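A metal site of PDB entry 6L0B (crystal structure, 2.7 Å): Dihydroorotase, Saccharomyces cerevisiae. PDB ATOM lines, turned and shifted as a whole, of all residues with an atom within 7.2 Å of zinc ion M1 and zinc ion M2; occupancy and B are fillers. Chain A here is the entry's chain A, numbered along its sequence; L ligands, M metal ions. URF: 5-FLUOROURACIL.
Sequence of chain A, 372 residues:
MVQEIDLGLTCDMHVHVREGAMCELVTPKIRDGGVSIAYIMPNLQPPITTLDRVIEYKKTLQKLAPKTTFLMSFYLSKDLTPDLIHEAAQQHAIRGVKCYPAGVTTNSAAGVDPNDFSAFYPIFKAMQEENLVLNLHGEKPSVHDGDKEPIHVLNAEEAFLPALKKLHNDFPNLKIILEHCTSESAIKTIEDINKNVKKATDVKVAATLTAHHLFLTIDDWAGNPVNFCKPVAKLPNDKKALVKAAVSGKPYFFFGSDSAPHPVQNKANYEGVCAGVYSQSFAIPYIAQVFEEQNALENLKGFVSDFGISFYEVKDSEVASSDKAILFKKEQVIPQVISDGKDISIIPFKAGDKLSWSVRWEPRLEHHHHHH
Of the 24 residues printed, 4 come within 4 Å of zinc ion M1. The nearest printed residue that does not touch zinc ion M1 is His 180 (4.5 Å).
O4 of the ligand sits at hydrogen-bond distance from NH1 of Arg 18 (2.7 Å). An oxygen (O4) of the ligand lies within hydrogen-bond range of the side-chain amide nitrogen (ND2) of Asn 43. A ring nitrogen (ND1) of His 16 is in hydrogen-bond range of an oxygen (O4) of the ligand, at 3.2 Å. The side-chain hydroxyl (OG1) of Thr 105 lies within hydrogen-bond range of a nitrogen (N1) of the ligand.
Zinc ion M1 is bound by a ring nitrogen (NE2) of His 16, a ring nitrogen (NE2) of His 14, OQ1 of KCX 98 and the side-chain carboxylate of Asp 258.
Zinc ion M2 is bound by ND1 of His 137 (2.1 Å), OQ2 of KCX 98 (2.1 Å), NE2 of His 180 (2.4 Å) and O2 of the ligand (2.4 Å).
ND1 of His 16 is in hydrogen-bond range of OD1 of Asn 43, at 3.0 Å. NE2 of His 137 lies within hydrogen-bond range of OE1 of Glu 139, at 2.9 Å. NZ of KCX 98 sits at hydrogen-bond distance from OH of Tyr 100, 3.4 Å away. N of His 137 is in hydrogen-bond range of O of Cys 99 (3.2 Å). OG of Ser 257 is in hydrogen-bond range of O of His 14, at 3.3 Å. SD of Met 41 lies within hydrogen-bond range of NZ of KCX 98 (3.6 Å). The backbone carbonyl oxygen (O) of Ser 259 lies within hydrogen-bond range of the backbone NH (N) of His 16 (3.3 Å).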
ATOM      1  N   HIS A  14       4.443 -15.100 -10.963  1.00  0.00           N
ATOM      2  CA  HIS A  14       4.485 -13.898 -10.132  1.00  0.00           C
ATOM      3  C   HIS A  14       4.135 -12.711 -11.032  1.00  0.00           C
ATOM      4  O   HIS A  14       5.021 -12.087 -11.615  1.00  0.00           O
ATOM      5  CB  HIS A  14       5.832 -13.710  -9.476  1.00  0.00           C
ATOM      6  CG  HIS A  14       5.816 -12.788  -8.304  1.00  0.00           C
ATOM      7  ND1 HIS A  14       6.271 -13.158  -7.061  1.00  0.00           N
ATOM      8  CD2 HIS A  14       5.396 -11.501  -8.175  1.00  0.00           C
ATOM      9  CE1 HIS A  14       6.149 -12.144  -6.217  1.00  0.00           C
ATOM     10  NE2 HIS A  14       5.626 -11.132  -6.876  1.00  0.00           N
ATOM     11  N   VAL A  15       2.863 -12.384 -11.110  1.00  0.00           N
ATOM     12  CA  VAL A  15       2.374 -11.375 -12.032  1.00  0.00           C
ATOM     13  C   VAL A  15       1.558 -10.365 -11.248  1.00  0.00           C
ATOM     14  O   VAL A  15       0.826 -10.722 -10.323  1.00  0.00           O
ATOM     15  CB  VAL A  15       1.545 -11.996 -13.164  1.00  0.00           C
ATOM     16  CG1 VAL A  15       0.990 -10.915 -14.072  1.00  0.00           C
ATOM     17  CG2 VAL A  15       2.354 -13.011 -13.968  1.00  0.00           C
ATOM     18  N   HIS A  16       1.736  -9.073 -11.565  1.00  0.00           N
ATOM     19  CA  HIS A  16       0.842  -8.012 -11.131  1.00  0.00           C
ATOM     20  C   HIS A  16       0.250  -7.307 -12.347  1.00  0.00           C
ATOM     21  O   HIS A  16       1.004  -6.906 -13.235  1.00  0.00           O
ATOM     22  CB  HIS A  16       1.566  -6.994 -10.217  1.00  0.00           C
ATOM     23  CG  HIS A  16       2.263  -7.605  -9.033  1.00  0.00           C
ATOM     24  ND1 HIS A  16       1.911  -7.313  -7.733  1.00  0.00           N
ATOM     25  CD2 HIS A  16       3.306  -8.468  -8.956  1.00  0.00           C
ATOM     26  CE1 HIS A  16       2.673  -8.000  -6.904  1.00  0.00           C
ATOM     27  NE2 HIS A  16       3.528  -8.712  -7.621  1.00  0.00           N
ATOM     28  N   ARG A  18      -2.756  -5.025 -11.818  1.00  0.00           N
ATOM     29  CA  ARG A  18      -3.489  -3.846 -11.325  1.00  0.00           C
ATOM     30  C   ARG A  18      -4.957  -3.950 -11.741  1.00  0.00           C
ATOM     31  O   ARG A  18      -5.514  -5.042 -11.874  1.00  0.00           O
ATOM     32  CB  ARG A  18      -2.803  -2.558 -11.788  1.00  0.00           C
ATOM     33  CG  ARG A  18      -1.268  -2.543 -11.745  1.00  0.00           C
ATOM     34  CD  ARG A  18      -0.678  -2.543 -10.318  1.00  0.00           C
ATOM     35  NE  ARG A  18       0.780  -2.328 -10.277  1.00  0.00           N
ATOM     36  CZ  ARG A  18       1.639  -2.818  -9.367  1.00  0.00           C
ATOM     37  NH1 ARG A  18       1.262  -3.613  -8.352  1.00  0.00           N
ATOM     38  NH2 ARG A  18       2.930  -2.530  -9.498  1.00  0.00           N
ATOM     39  N   MET A  41      -1.363 -11.775  -8.645  1.00  0.00           N
ATOM     40  CA  MET A  41      -1.091 -11.371  -7.272  1.00  0.00           C
ATOM     41  C   MET A  41      -2.202 -10.481  -6.702  1.00  0.00           C
ATOM     42  O   MET A  41      -2.965  -9.864  -7.458  1.00  0.00           O
ATOM     43  CB  MET A  41       0.260 -10.654  -7.189  1.00  0.00           C
ATOM     44  CG  MET A  41       1.457 -11.620  -7.200  1.00  0.00           C
ATOM     45  SD  MET A  41       1.457 -12.886  -5.899  1.00  0.00           S
ATOM     46  CE  MET A  41       2.955 -13.809  -6.339  1.00  0.00           C
ATOM     47  N   ASN A  43      -2.315  -7.743  -4.388  1.00  0.00           N
ATOM     48  CA  ASN A  43      -2.069  -6.476  -3.696  1.00  0.00           C
ATOM     49  C   ASN A  43      -2.687  -5.304  -4.454  1.00  0.00           C
ATOM     50  O   ASN A  43      -2.008  -4.371  -4.913  1.00  0.00           O
ATOM     51  CB  ASN A  43      -0.568  -6.297  -3.494  1.00  0.00           C
ATOM     52  CG  ASN A  43       0.168  -6.116  -4.801  1.00  0.00           C
ATOM     53  OD1 ASN A  43      -0.338  -6.541  -5.851  1.00  0.00           O
ATOM     54  ND2 ASN A  43       1.332  -5.463  -4.756  1.00  0.00           N
ATOM     55  N   KCX A  98      -0.797 -15.034  -0.874  1.00  0.00           N
ATOM     56  CA  KCX A  98       0.454 -14.285  -0.921  1.00  0.00           C
ATOM     57  CB  KCX A  98       0.538 -13.377  -2.163  1.00  0.00           C
ATOM     58  CG  KCX A  98       1.725 -12.399  -2.160  1.00  0.00           C
ATOM     59  CD  KCX A  98       3.039 -13.192  -2.217  1.00  0.00           C
ATOM     60  CE  KCX A  98       4.230 -12.317  -2.505  1.00  0.00           C
ATOM     61  NZ  KCX A  98       3.715 -11.369  -3.502  1.00  0.00           N
ATOM     62  C   KCX A  98       0.571 -13.427   0.308  1.00  0.00           C
ATOM     63  O   KCX A  98      -0.318 -12.643   0.635  1.00  0.00           O
ATOM     64  CX  KCX A  98       4.471 -10.478  -4.129  1.00  0.00           C
ATOM     65  OQ1 KCX A  98       3.940  -9.722  -4.948  1.00  0.00           O
ATOM     66  OQ2 KCX A  98       5.690 -10.417  -3.929  1.00  0.00           O
ATOM     67  N   CYS A  99       1.696 -13.611   0.976  1.00  0.00           N
ATOM     68  CA  CYS A  99       1.993 -12.888   2.186  1.00  0.00           C
ATOM     69  C   CYS A  99       2.882 -11.683   1.913  1.00  0.00           C
ATOM     70  O   CYS A  99       3.931 -11.813   1.289  1.00  0.00           O
ATOM     71  CB  CYS A  99       2.676 -13.817   3.196  1.00  0.00           C
ATOM     72  SG  CYS A  99       3.320 -12.907   4.637  1.00  0.00           S
ATOM     73  N   TYR A 100       2.465 -10.502   2.390  1.00  0.00           N
ATOM     74  CA  TYR A 100       3.287  -9.290   2.337  1.00  0.00           C
ATOM     75  C   TYR A 100       3.650  -8.873   3.753  1.00  0.00           C
ATOM     76  O   TYR A 100       2.741  -8.503   4.526  1.00  0.00           O
ATOM     77  CB  TYR A 100       2.555  -8.132   1.633  1.00  0.00           C
ATOM     78  CG  TYR A 100       2.283  -8.317   0.148  1.00  0.00           C
ATOM     79  CD1 TYR A 100       3.228  -7.990  -0.828  1.00  0.00           C
ATOM     80  CD2 TYR A 100       1.060  -8.827  -0.276  1.00  0.00           C
ATOM     81  CE1 TYR A 100       2.965  -8.165  -2.187  1.00  0.00           C
ATOM     82  CE2 TYR A 100       0.788  -9.008  -1.626  1.00  0.00           C
ATOM     83  CZ  TYR A 100       1.722  -8.673  -2.575  1.00  0.00           C
ATOM     84  OH  TYR A 100       1.401  -8.881  -3.893  1.00  0.00           O
ATOM     85  N   VAL A 104       6.829  -3.314   3.480  1.00  0.00           N
ATOM     86  CA  VAL A 104       8.086  -3.559   2.780  1.00  0.00           C
ATOM     87  C   VAL A 104       7.988  -3.296   1.286  1.00  0.00           C
ATOM     88  O   VAL A 104       9.030  -3.154   0.635  1.00  0.00           O
ATOM     89  CB  VAL A 104       8.594  -4.993   2.991  1.00  0.00           C
ATOM     90  CG1 VAL A 104       8.763  -5.293   4.467  1.00  0.00           C
ATOM     91  CG2 VAL A 104       7.650  -6.003   2.357  1.00  0.00           C
ATOM     92  N   THR A 105       6.790  -3.205   0.715  1.00  0.00           N
ATOM     93  CA  THR A 105       6.648  -3.030  -0.727  1.00  0.00           C
ATOM     94  C   THR A 105       5.293  -2.398  -1.029  1.00  0.00           C
ATOM     95  O   THR A 105       4.547  -2.025  -0.116  1.00  0.00           O
ATOM     96  CB  THR A 105       6.807  -4.390  -1.429  1.00  0.00           C
ATOM     97  OG1 THR A 105       6.708  -4.213  -2.839  1.00  0.00           O
ATOM     98  CG2 THR A 105       5.712  -5.344  -0.958  1.00  0.00           C
ATOM     99  N   THR A 106       4.926  -2.365  -2.314  1.00  0.00           N
ATOM    100  CA  THR A 106       3.699  -1.701  -2.774  1.00  0.00           C
ATOM    101  C   THR A 106       2.466  -2.362  -2.185  1.00  0.00           C
ATOM    102  O   THR A 106       2.318  -3.581  -2.261  1.00  0.00           O
ATOM    103  CB  THR A 106       3.585  -1.781  -4.297  1.00  0.00           C
ATOM    104  OG1 THR A 106       4.661  -1.087  -4.933  1.00  0.00           O
ATOM    105  CG2 THR A 106       2.273  -1.198  -4.773  1.00  0.00           C
ATOM    106  N   LEU A 136       5.513 -16.213  -0.499  1.00  0.00           N
ATOM    107  CA  LEU A 136       6.164 -15.413   0.531  1.00  0.00           C
ATOM    108  C   LEU A 136       7.001 -14.330  -0.100  1.00  0.00           C
ATOM    109  O   LEU A 136       7.976 -14.633  -0.809  1.00  0.00           O
ATOM    110  CB  LEU A 136       7.072 -16.289   1.403  1.00  0.00           C
ATOM    111  CG  LEU A 136       6.381 -17.369   2.223  1.00  0.00           C
ATOM    112  CD1 LEU A 136       7.444 -18.078   3.007  1.00  0.00           C
ATOM    113  CD2 LEU A 136       5.330 -16.757   3.130  1.00  0.00           C
ATOM    114  N   HIS A 137       6.699 -13.076   0.221  1.00  0.00           N
ATOM    115  CA  HIS A 137       7.639 -11.975   0.007  1.00  0.00           C
ATOM    116  C   HIS A 137       8.548 -11.923   1.223  1.00  0.00           C
ATOM    117  O   HIS A 137       8.281 -11.212   2.178  1.00  0.00           O
ATOM    118  CB  HIS A 137       6.933 -10.642  -0.191  1.00  0.00           C
ATOM    119  CG  HIS A 137       7.870  -9.497  -0.479  1.00  0.00           C
ATOM    120  ND1 HIS A 137       7.812  -8.766  -1.645  1.00  0.00           N
ATOM    121  CD2 HIS A 137       8.877  -8.954   0.257  1.00  0.00           C
ATOM    122  CE1 HIS A 137       8.731  -7.822  -1.621  1.00  0.00           C
ATOM    123  NE2 HIS A 137       9.386  -7.912  -0.471  1.00  0.00           N
ATOM    124  N   GLY A 138       9.646 -12.658   1.154  1.00  0.00           N
ATOM    125  CA  GLY A 138      10.498 -12.837   2.309  1.00  0.00           C
ATOM    126  C   GLY A 138      11.438 -11.695   2.643  1.00  0.00           C
ATOM    127  O   GLY A 138      12.604 -11.678   2.229  1.00  0.00           O
ATOM    128  N   GLU A 139      10.936 -10.715   3.355  1.00  0.00           N
ATOM    129  CA  GLU A 139      11.778  -9.619   3.814  1.00  0.00           C
ATOM    130  C   GLU A 139      11.236  -9.200   5.172  1.00  0.00           C
ATOM    131  O   GLU A 139      10.030  -9.015   5.329  1.00  0.00           O
ATOM    132  CB  GLU A 139      11.786  -8.443   2.833  1.00  0.00           C
ATOM    133  CG  GLU A 139      12.641  -8.681   1.604  1.00  0.00           C
ATOM    134  CD  GLU A 139      12.965  -7.420   0.855  1.00  0.00           C
ATOM    135  OE1 GLU A 139      12.105  -6.918   0.073  1.00  0.00           O
ATOM    136  OE2 GLU A 139      14.092  -6.910   1.077  1.00  0.00           O
ATOM    137  N   GLU A 179       9.360 -16.145  -2.879  1.00  0.00           N
ATOM    138  CA  GLU A 179       9.243 -15.360  -4.102  1.00  0.00           C
ATOM    139  C   GLU A 179      10.458 -14.486  -4.345  1.00  0.00           C
ATOM    140  O   GLU A 179      11.078 -13.971  -3.397  1.00  0.00           O
ATOM    141  CB  GLU A 179       8.000 -14.451  -4.064  1.00  0.00           C
ATOM    142  CG  GLU A 179       6.702 -15.198  -3.995  1.00  0.00           C
ATOM    143  CD  GLU A 179       6.296 -15.793  -5.327  1.00  0.00           C
ATOM    144  OE1 GLU A 179       6.717 -15.288  -6.387  1.00  0.00           O
ATOM    145  OE2 GLU A 179       5.536 -16.777  -5.297  1.00  0.00           O
ATOM    146  N   HIS A 180      10.723 -14.235  -5.633  1.00  0.00           N
ATOM    147  CA  HIS A 180      11.814 -13.401  -6.142  1.00  0.00           C
ATOM    148  C   HIS A 180      13.063 -13.410  -5.263  1.00  0.00           C
ATOM    149  O   HIS A 180      13.371 -12.402  -4.610  1.00  0.00           O
ATOM    150  CB  HIS A 180      11.327 -11.949  -6.364  1.00  0.00           C
ATOM    151  CG  HIS A 180      10.438 -11.395  -5.282  1.00  0.00           C
ATOM    152  ND1 HIS A 180      10.666 -11.618  -3.938  1.00  0.00           N
ATOM    153  CD2 HIS A 180       9.366 -10.568  -5.356  1.00  0.00           C
ATOM    154  CE1 HIS A 180       9.734 -10.997  -3.235  1.00  0.00           C
ATOM    155  NE2 HIS A 180       8.941 -10.354  -4.068  1.00  0.00           N
ATOM    156  N   LYS A 230      11.457  -4.198  -4.936  1.00  0.00           N
ATOM    157  CA  LYS A 230      11.655  -4.911  -3.675  1.00  0.00           C
ATOM    158  C   LYS A 230      11.509  -6.407  -3.938  1.00  0.00           C
ATOM    159  O   LYS A 230      10.619  -6.794  -4.708  1.00  0.00           O
ATOM    160  CB  LYS A 230      10.658  -4.455  -2.597  1.00  0.00           C
ATOM    161  CG  LYS A 230      10.771  -2.983  -2.187  1.00  0.00           C
ATOM    162  CD  LYS A 230      12.159  -2.647  -1.701  1.00  0.00           C
ATOM    163  CE  LYS A 230      12.463  -3.253  -0.343  1.00  0.00           C
ATOM    164  NZ  LYS A 230      11.894  -2.440   0.772  1.00  0.00           N
ATOM    165  N   PRO A 231      12.428  -7.266  -3.445  1.00  0.00           N
ATOM    166  CA  PRO A 231      13.653  -6.864  -2.740  1.00  0.00           C
ATOM    167  C   PRO A 231      14.632  -6.217  -3.718  1.00  0.00           C
ATOM    168  O   PRO A 231      14.616  -6.541  -4.909  1.00  0.00           O
ATOM    169  CB  PRO A 231      14.215  -8.175  -2.200  1.00  0.00           C
ATOM    170  CG  PRO A 231      13.097  -9.155  -2.290  1.00  0.00           C
ATOM    171  CD  PRO A 231      12.229  -8.720  -3.427  1.00  0.00           C
ATOM    172  N   SER A 257       8.040 -13.468 -12.861  1.00  0.00           N
ATOM    173  CA  SER A 257       8.644 -12.202 -13.266  1.00  0.00           C
ATOM    174  C   SER A 257       8.532 -11.105 -12.206  1.00  0.00           C
ATOM    175  O   SER A 257       9.406 -10.241 -12.136  1.00  0.00           O
ATOM    176  CB  SER A 257       7.980 -11.694 -14.549  1.00  0.00           C
ATOM    177  OG  SER A 257       6.755 -11.029 -14.223  1.00  0.00           O
ATOM    178  N   ASP A 258       7.485 -11.105 -11.393  1.00  0.00           N
ATOM    179  CA  ASP A 258       7.113  -9.928 -10.602  1.00  0.00           C
ATOM    180  C   ASP A 258       7.141  -8.672 -11.467  1.00  0.00           C
ATOM    181  O   ASP A 258       7.642  -7.622 -11.079  1.00  0.00           O
ATOM    182  CB  ASP A 258       8.014  -9.767  -9.376  1.00  0.00           C
ATOM    183  CG  ASP A 258       7.582  -8.615  -8.453  1.00  0.00           C
ATOM    184  OD1 ASP A 258       6.398  -8.195  -8.485  1.00  0.00           O
ATOM    185  OD2 ASP A 258       8.419  -8.144  -7.671  1.00  0.00           O
ATOM    186  N   SER A 259       6.608  -8.788 -12.673  1.00  0.00           N
ATOM    187  CA  SER A 259       6.405  -7.573 -13.433  1.00  0.00           C
ATOM    188  C   SER A 259       5.399  -6.736 -12.664  1.00  0.00           C
ATOM    189  O   SER A 259       4.270  -7.177 -12.430  1.00  0.00           O
ATOM    190  CB  SER A 259       5.959  -7.919 -14.853  1.00  0.00           C
ATOM    191  OG  SER A 259       5.749  -6.751 -15.639  1.00  0.00           O
ATOM    192  N   ALA A 260       5.824  -5.551 -12.198  1.00  0.00           N
ATOM    193  CA  ALA A 260       5.015  -4.664 -11.345  1.00  0.00           C
ATOM    194  C   ALA A 260       4.899  -3.287 -12.003  1.00  0.00           C
ATOM    195  O   ALA A 260       5.731  -2.404 -11.777  1.00  0.00           O
ATOM    196  CB  ALA A 260       5.628  -4.550  -9.954  1.00  0.00           C
HETATM  197  N1  URF L   1       7.105  -4.773  -5.681  1.00  0.00           N
HETATM  198  C2  URF L   1       6.276  -5.954  -5.332  1.00  0.00           C
HETATM  199  N3  URF L   1       4.827  -5.872  -5.676  1.00  0.00           N
HETATM  200  C4  URF L   1       4.278  -4.679  -6.332  1.00  0.00           C
HETATM  201  C5  URF L   1       5.121  -3.526  -6.651  1.00  0.00           C
HETATM  202  C6  URF L   1       6.516  -3.610  -6.307  1.00  0.00           C
HETATM  203  O2  URF L   1       6.752  -6.918  -4.786  1.00  0.00           O
HETATM  204  O4  URF L   1       3.143  -4.563  -6.650  1.00  0.00           O
HETATM  205  F5  URF L   1       4.493  -2.443  -7.248  1.00  0.00           F
HETATM  206 ZN    ZN M   1       5.340  -8.945  -6.541  1.00  0.00          ZN
HETATM  207 ZN    ZN M   2       7.145  -8.914  -3.589  1.00  0.00          ZN
